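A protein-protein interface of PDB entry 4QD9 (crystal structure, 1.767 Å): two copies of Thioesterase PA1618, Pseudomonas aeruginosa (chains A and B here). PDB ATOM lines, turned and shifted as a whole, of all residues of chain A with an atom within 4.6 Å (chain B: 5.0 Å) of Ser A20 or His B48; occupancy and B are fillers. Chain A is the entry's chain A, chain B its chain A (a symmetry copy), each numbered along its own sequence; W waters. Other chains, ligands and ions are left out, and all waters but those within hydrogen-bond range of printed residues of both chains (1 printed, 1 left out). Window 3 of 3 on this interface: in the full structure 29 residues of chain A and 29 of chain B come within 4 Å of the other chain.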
ATOM      1  N   GLN A  17      15.864  -3.866 -15.392  1.00  0.00           N
ATOM      2  CA  GLN A  17      15.038  -4.082 -14.201  1.00  0.00           C
ATOM      3  C   GLN A  17      15.610  -5.100 -13.218  1.00  0.00           C
ATOM      4  O   GLN A  17      15.043  -5.315 -12.144  1.00  0.00           O
ATOM      5  CB  GLN A  17      13.640  -4.547 -14.606  1.00  0.00           C
ATOM      6  CG  GLN A  17      12.824  -3.551 -15.389  1.00  0.00           C
ATOM      7  CD  GLN A  17      11.382  -3.998 -15.508  1.00  0.00           C
ATOM      8  OE1 GLN A  17      10.462  -3.293 -15.085  1.00  0.00           O
ATOM      9  NE2 GLN A  17      11.174  -5.175 -16.087  1.00  0.00           N
ATOM     10  N   LYS A  18      16.717  -5.737 -13.591  1.00  0.00           N
ATOM     11  CA  LYS A  18      17.352  -6.745 -12.743  1.00  0.00           C
ATOM     12  C   LYS A  18      17.628  -6.205 -11.338  1.00  0.00           C
ATOM     13  O   LYS A  18      18.134  -5.093 -11.188  1.00  0.00           O
ATOM     14  CB  LYS A  18      18.655  -7.216 -13.398  1.00  0.00           C
ATOM     15  CG  LYS A  18      19.254  -8.472 -12.784  1.00  0.00           C
ATOM     16  CD  LYS A  18      20.613  -8.782 -13.404  1.00  0.00           C
ATOM     17  CE  LYS A  18      21.212 -10.065 -12.843  1.00  0.00           C
ATOM     18  NZ  LYS A  18      22.440 -10.470 -13.594  1.00  0.00           N
ATOM     19  N   ASN A  19      17.272  -6.983 -10.317  1.00  0.00           N
ATOM     20  CA  ASN A  19      17.424  -6.573  -8.916  1.00  0.00           C
ATOM     21  C   ASN A  19      16.628  -5.328  -8.554  1.00  0.00           C
ATOM     22  O   ASN A  19      17.104  -4.480  -7.794  1.00  0.00           O
ATOM     23  CB  ASN A  19      18.891  -6.329  -8.541  1.00  0.00           C
ATOM     24  CG  ASN A  19      19.767  -7.533  -8.775  1.00  0.00           C
ATOM     25  OD1 ASN A  19      19.341  -8.676  -8.599  1.00  0.00           O
ATOM     26  ND2 ASN A  19      21.012  -7.281  -9.171  1.00  0.00           N
ATOM     27  N   SER A  20      15.431  -5.200  -9.113  1.00  0.00           N
ATOM     28  CA  SER A  20      14.548  -4.111  -8.729  1.00  0.00           C
ATOM     29  C   SER A  20      13.126  -4.660  -8.702  1.00  0.00           C
ATOM     30  O   SER A  20      12.899  -5.825  -9.036  1.00  0.00           O
ATOM     31  CB  SER A  20      14.662  -2.934  -9.692  1.00  0.00           C
ATOM     32  OG  SER A  20      14.155  -3.283 -10.960  1.00  0.00           O
ATOM     33  N   ILE A  21      12.172  -3.838  -8.288  1.00  0.00           N
ATOM     34  CA  ILE A  21      10.814  -4.344  -8.076  1.00  0.00           C
ATOM     35  C   ILE A  21      10.168  -4.821  -9.380  1.00  0.00           C
ATOM     36  O   ILE A  21       9.387  -5.773  -9.379  1.00  0.00           O
ATOM     37  CB  ILE A  21       9.929  -3.290  -7.356  1.00  0.00           C
ATOM     38  CG1 ILE A  21       8.552  -3.866  -7.007  1.00  0.00           C
ATOM     39  CG2 ILE A  21       9.761  -2.054  -8.215  1.00  0.00           C
ATOM     40  CD1 ILE A  21       7.743  -2.952  -6.083  1.00  0.00           C
ATOM     41  N   GLY A  22      10.505  -4.171 -10.492  1.00  0.00           N
ATOM     42  CA  GLY A  22       9.964  -4.557 -11.789  1.00  0.00           C
ATOM     43  C   GLY A  22      10.243  -6.002 -12.174  1.00  0.00           C
ATOM     44  O   GLY A  22       9.380  -6.696 -12.723  1.00  0.00           O
ATOM     45  N   ASP A  23      11.453  -6.461 -11.880  1.00  0.00           N
ATOM     46  CA  ASP A  23      11.831  -7.845 -12.143  1.00  0.00           C
ATOM     47  C   ASP A  23      11.054  -8.770 -11.206  1.00  0.00           C
ATOM     48  O   ASP A  23      10.529  -9.803 -11.622  1.00  0.00           O
ATOM     49  CB  ASP A  23      13.338  -8.003 -11.912  1.00  0.00           C
ATOM     50  CG  ASP A  23      13.905  -9.262 -12.543  1.00  0.00           C
ATOM     51  OD1 ASP A  23      13.418  -9.667 -13.625  1.00  0.00           O
ATOM     52  OD2 ASP A  23      14.851  -9.835 -11.955  1.00  0.00           O
ATOM     53  N   LEU A  24      10.978  -8.379  -9.937  1.00  0.00           N
ATOM     54  CA  LEU A  24      10.259  -9.134  -8.921  1.00  0.00           C
ATOM     55  C   LEU A  24       8.787  -9.345  -9.284  1.00  0.00           C
ATOM     56  O   LEU A  24       8.242 -10.429  -9.071  1.00  0.00           O
ATOM     57  CB  LEU A  24      10.379  -8.430  -7.562  1.00  0.00           C
ATOM     58  CG  LEU A  24      10.077  -9.301  -6.346  1.00  0.00           C
ATOM     59  CD1 LEU A  24      11.123 -10.385  -6.247  1.00  0.00           C
ATOM     60  CD2 LEU A  24      10.033  -8.483  -5.059  1.00  0.00           C
ATOM     61  N   VAL B  43      13.661  -0.986   2.208  1.00  0.00           N
ATOM     62  CA  VAL B  43      14.139  -0.314   1.013  1.00  0.00           C
ATOM     63  C   VAL B  43      15.360  -1.087   0.550  1.00  0.00           C
ATOM     64  O   VAL B  43      16.467  -0.879   1.055  1.00  0.00           O
ATOM     65  CB  VAL B  43      14.524   1.163   1.273  1.00  0.00           C
ATOM     66  CG1 VAL B  43      14.943   1.845  -0.030  1.00  0.00           C
ATOM     67  CG2 VAL B  43      13.361   1.935   1.904  1.00  0.00           C
ATOM     68  N   ASP B  44      15.136  -2.013  -0.376  1.00  0.00           N
ATOM     69  CA  ASP B  44      16.214  -2.815  -0.957  1.00  0.00           C
ATOM     70  C   ASP B  44      15.852  -3.266  -2.375  1.00  0.00           C
ATOM     71  O   ASP B  44      14.967  -2.676  -3.008  1.00  0.00           O
ATOM     72  CB  ASP B  44      16.601  -4.002  -0.051  1.00  0.00           C
ATOM     73  CG  ASP B  44      15.437  -4.936   0.255  1.00  0.00           C
ATOM     74  OD1 ASP B  44      14.512  -5.078  -0.572  1.00  0.00           O
ATOM     75  OD2 ASP B  44      15.458  -5.560   1.334  1.00  0.00           O
ATOM     76  N   SER B  45      16.520  -4.305  -2.874  1.00  0.00           N
ATOM     77  CA  SER B  45      16.300  -4.746  -4.250  1.00  0.00           C
ATOM     78  C   SER B  45      14.857  -5.161  -4.529  1.00  0.00           C
ATOM     79  O   SER B  45      14.430  -5.167  -5.683  1.00  0.00           O
ATOM     80  CB  SER B  45      17.259  -5.890  -4.625  1.00  0.00           C
ATOM     81  OG  SER B  45      16.982  -7.044  -3.853  1.00  0.00           O
ATOM     82  N   ARG B  46      14.102  -5.511  -3.489  1.00  0.00           N
ATOM     83  CA  ARG B  46      12.704  -5.892  -3.691  1.00  0.00           C
ATOM     84  C   ARG B  46      11.847  -4.687  -4.042  1.00  0.00           C
ATOM     85  O   ARG B  46      10.840  -4.819  -4.734  1.00  0.00           O
ATOM     86  CB  ARG B  46      12.131  -6.566  -2.442  1.00  0.00           C
ATOM     87  CG  ARG B  46      12.688  -7.947  -2.157  1.00  0.00           C
ATOM     88  CD  ARG B  46      12.281  -8.399  -0.768  1.00  0.00           C
ATOM     89  NE  ARG B  46      13.051  -7.730   0.282  1.00  0.00           N
ATOM     90  CZ  ARG B  46      12.891  -7.945   1.587  1.00  0.00           C
ATOM     91  NH1 ARG B  46      11.976  -8.801   2.012  1.00  0.00           N
ATOM     92  NH2 ARG B  46      13.648  -7.303   2.470  1.00  0.00           N
ATOM     93  N   THR B  47      12.253  -3.514  -3.563  1.00  0.00           N
ATOM     94  CA  THR B  47      11.429  -2.320  -3.676  1.00  0.00           C
ATOM     95  C   THR B  47      12.133  -1.163  -4.401  1.00  0.00           C
ATOM     96  O   THR B  47      11.544  -0.105  -4.585  1.00  0.00           O
ATOM     97  CB  THR B  47      10.967  -1.850  -2.280  1.00  0.00           C
ATOM     98  OG1 THR B  47      12.111  -1.659  -1.441  1.00  0.00           O
ATOM     99  CG2 THR B  47      10.056  -2.902  -1.626  1.00  0.00           C
ATOM    100  N   HIS B  48      13.388  -1.355  -4.809  1.00  0.00           N
ATOM    101  CA  HIS B  48      14.090  -0.342  -5.612  1.00  0.00           C
ATOM    102  C   HIS B  48      13.533  -0.187  -7.026  1.00  0.00           C
ATOM    103  O   HIS B  48      12.971  -1.131  -7.588  1.00  0.00           O
ATOM    104  CB  HIS B  48      15.573  -0.718  -5.768  1.00  0.00           C
ATOM    105  CG  HIS B  48      16.418  -0.407  -4.576  1.00  0.00           C
ATOM    106  ND1 HIS B  48      17.665  -0.969  -4.391  1.00  0.00           N
ATOM    107  CD2 HIS B  48      16.212   0.412  -3.518  1.00  0.00           C
ATOM    108  CE1 HIS B  48      18.186  -0.516  -3.265  1.00  0.00           C
ATOM    109  NE2 HIS B  48      17.326   0.324  -2.716  1.00  0.00           N
ATOM    110  N   GLN B  49      13.705   0.999  -7.612  1.00  0.00           N
ATOM    111  CA  GLN B  49      13.584   1.157  -9.068  1.00  0.00           C
ATOM    112  C   GLN B  49      14.980   0.910  -9.680  1.00  0.00           C
ATOM    113  O   GLN B  49      15.925   0.632  -8.929  1.00  0.00           O
ATOM    114  CB  GLN B  49      12.973   2.512  -9.448  1.00  0.00           C
ATOM    115  CG  GLN B  49      13.287   3.685  -8.534  1.00  0.00           C
ATOM    116  CD  GLN B  49      14.588   4.370  -8.884  1.00  0.00           C
ATOM    117  OE1 GLN B  49      15.636   3.731  -8.954  1.00  0.00           O
ATOM    118  NE2 GLN B  49      14.530   5.682  -9.097  1.00  0.00           N
ATOM    119  N   PRO B  50      15.121   0.970 -11.025  1.00  0.00           N
ATOM    120  CA  PRO B  50      16.427   0.549 -11.567  1.00  0.00           C
ATOM    121  C   PRO B  50      17.636   1.411 -11.194  1.00  0.00           C
ATOM    122  O   PRO B  50      18.762   1.003 -11.486  1.00  0.00           O
ATOM    123  CB  PRO B  50      16.206   0.608 -13.085  1.00  0.00           C
ATOM    124  CG  PRO B  50      14.745   0.361 -13.249  1.00  0.00           C
ATOM    125  CD  PRO B  50      14.130   1.131 -12.107  1.00  0.00           C
ATOM    126  N   GLY B  52      18.398   2.411  -8.039  1.00  0.00           N
ATOM    127  CA  GLY B  52      18.819   2.161  -6.675  1.00  0.00           C
ATOM    128  C   GLY B  52      18.068   2.944  -5.611  1.00  0.00           C
ATOM    129  O   GLY B  52      18.448   2.907  -4.439  1.00  0.00           O
ATOM    130  N   LEU B  53      17.015   3.659  -6.016  1.00  0.00           N
ATOM    131  CA  LEU B  53      16.161   4.388  -5.076  1.00  0.00           C
ATOM    132  C   LEU B  53      14.850   3.632  -4.877  1.00  0.00           C
ATOM    133  O   LEU B  53      14.449   2.837  -5.719  1.00  0.00           O
ATOM    134  CB  LEU B  53      15.825   5.777  -5.611  1.00  0.00           C
ATOM    135  CG  LEU B  53      16.902   6.836  -5.797  1.00  0.00           C
ATOM    136  CD1 LEU B  53      16.262   8.121  -6.324  1.00  0.00           C
ATOM    137  CD2 LEU B  53      17.582   7.095  -4.498  1.00  0.00           C
ATOM    138  N   LEU B  54      14.184   3.867  -3.755  1.00  0.00           N
ATOM    139  CA  LEU B  54      12.868   3.276  -3.537  1.00  0.00           C
ATOM    140  C   LEU B  54      11.930   3.661  -4.673  1.00  0.00           C
ATOM    141  O   LEU B  54      11.791   4.846  -4.999  1.00  0.00           O
ATOM    142  CB  LEU B  54      12.305   3.759  -2.189  1.00  0.00           C
ATOM    143  CG  LEU B  54      10.878   3.351  -1.834  1.00  0.00           C
ATOM    144  CD1 LEU B  54      10.798   1.843  -1.685  1.00  0.00           C
ATOM    145  CD2 LEU B  54      10.464   4.047  -0.544  1.00  0.00           C
ATOM    146  N   HIS B  55      11.274   2.662  -5.267  1.00  0.00           N
ATOM    147  CA  HIS B  55      10.313   2.871  -6.359  1.00  0.00           C
ATOM    148  C   HIS B  55       9.111   3.638  -5.804  1.00  0.00           C
ATOM    149  O   HIS B  55       8.570   3.289  -4.744  1.00  0.00           O
ATOM    150  CB  HIS B  55       9.885   1.498  -6.916  1.00  0.00           C
ATOM    151  CG  HIS B  55       9.202   1.540  -8.248  1.00  0.00           C
ATOM    152  ND1 HIS B  55       7.995   2.173  -8.453  1.00  0.00           N
ATOM    153  CD2 HIS B  55       9.530   0.968  -9.433  1.00  0.00           C
ATOM    154  CE1 HIS B  55       7.623   2.017  -9.713  1.00  0.00           C
ATOM    155  NE2 HIS B  55       8.533   1.280 -10.328  1.00  0.00           N
ATOM    156  N   ARG B  96      17.368   5.255  -0.169  1.00  0.00           N
ATOM    157  CA  ARG B  96      18.237   4.236  -0.780  1.00  0.00           C
ATOM    158  C   ARG B  96      18.316   2.950   0.033  1.00  0.00           C
ATOM    159  O   ARG B  96      18.530   1.872  -0.518  1.00  0.00           O
ATOM    160  CB  ARG B  96      19.663   4.775  -0.999  1.00  0.00           C
ATOM    161  CG  ARG B  96      19.814   5.690  -2.197  1.00  0.00           C
ATOM    162  CD  ARG B  96      21.276   5.819  -2.643  1.00  0.00           C
ATOM    163  NE  ARG B  96      21.425   6.801  -3.715  1.00  0.00           N
ATOM    164  CZ  ARG B  96      21.252   6.537  -5.008  1.00  0.00           C
ATOM    165  NH1 ARG B  96      20.927   5.312  -5.407  1.00  0.00           N
ATOM    166  NH2 ARG B  96      21.404   7.500  -5.907  1.00  0.00           N
ATOM    167  N   SER B  97      18.173   3.054   1.347  1.00  0.00           N
ATOM    168  CA  SER B  97      18.275   1.862   2.193  1.00  0.00           C
ATOM    169  C   SER B  97      17.504   2.035   3.493  1.00  0.00           C
ATOM    170  O   SER B  97      16.839   3.060   3.694  1.00  0.00           O
ATOM    171  CB  SER B  97      19.744   1.540   2.495  1.00  0.00           C
ATOM    172  OG  SER B  97      20.358   2.646   3.130  1.00  0.00           O
HETATM  173  O   HOH W   1      18.715  -2.743  -6.289  1.00  0.00           O
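Water W1 bridges ND1 of His B48 (2.8 Å) and O of Asn A19 (2.8 Å).
No position is printed for both chains. Of the 9 pairs that touch across the chains among the printed residues, none has its exchanged pair printed and touching as well.
N of Ile A21 is in hydrogen-bond range of O of His B48 (2.9 Å). The backbone carbonyl oxygen (O) of Asn A19 lies close to the backbone carbonyl oxygen (O) of Ser B45.
Among the printed residues, merely in contact across the chains: Ser A20 with Ser B45 (3.2 Å), Ser A20 with His B48 (3.2 Å), Ser A20 with Gln B49 (3.9 Å), Ile A21 with Ser B45 (3.7 Å), Ile A21 with Arg B46 (3.2 Å), Ile A21 with His B55 (3.3 Å) and Leu A24 with Arg B46 (3.8 Å).
A ring nitrogen (ND1) of His B48 sits close to the backbone carbonyl oxygen of Asp B44, at 3.5 Å. O of Thr B47 lies within hydrogen-bond range of N of His B55 (2.9 Å). A ring nitrogen (NE2) of His B48 sits at hydrogen-bond distance from the backbone carbonyl oxygen (O) of Gly B52 (3.3 Å). NE2 of His B48 lies within hydrogen-bond range of O of Arg B96, at 2.9 Å. The side-chain amide oxygen of Gln B49 is in hydrogen-bond range of the backbone NH of Gly B52, 3.2 Å away. OE1 of Gln B49 is in hydrogen-bond range of N of Leu B53 (3.2 Å).
Of the 14 printed residues of chain B, 5 touch a printed residue of chain A. Printed residues of chain B that touch a printed residue of chain A: Ser B45, Arg B46, His B48, Gln B49 and His B55. Of the 8 printed residues of chain A, 4 touch a printed residue of chain B. Among the printed residues, no Asp or Glu carboxylate lies within 4 Å of a Lys or Arg side-chain nitrogen of the other chain.
Ser A20 touches three residues of chain B. His B48 touches just these residues of chain A: Ser A20 (3.2 Å) and Ile A21 (2.9 Å). Of the printed residues of chain A, Gln B49 touches Ser A20. Of the printed residues of chain A, Ser B45 touches Asn A19 (3.5 Å), Ser A20 (3.2 Å) and Ile A21 (3.7 Å). Printed residues of chain B within 4 Å of Ile A21: Ser B45, Arg B46, His B48 and His B55. Of the printed residues of chain A, His B55 touches Ile A21. Thr B47 touches none of the printed residues of chain A. Val B43 touches none of the printed residues of chain A. The nearest residue of chain A that does not touch His B48 is Asn A19 (4.5 Å). The nearest printed residue of chain A that does not touch Gln B49 is Ile A21 (5.0 Å).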
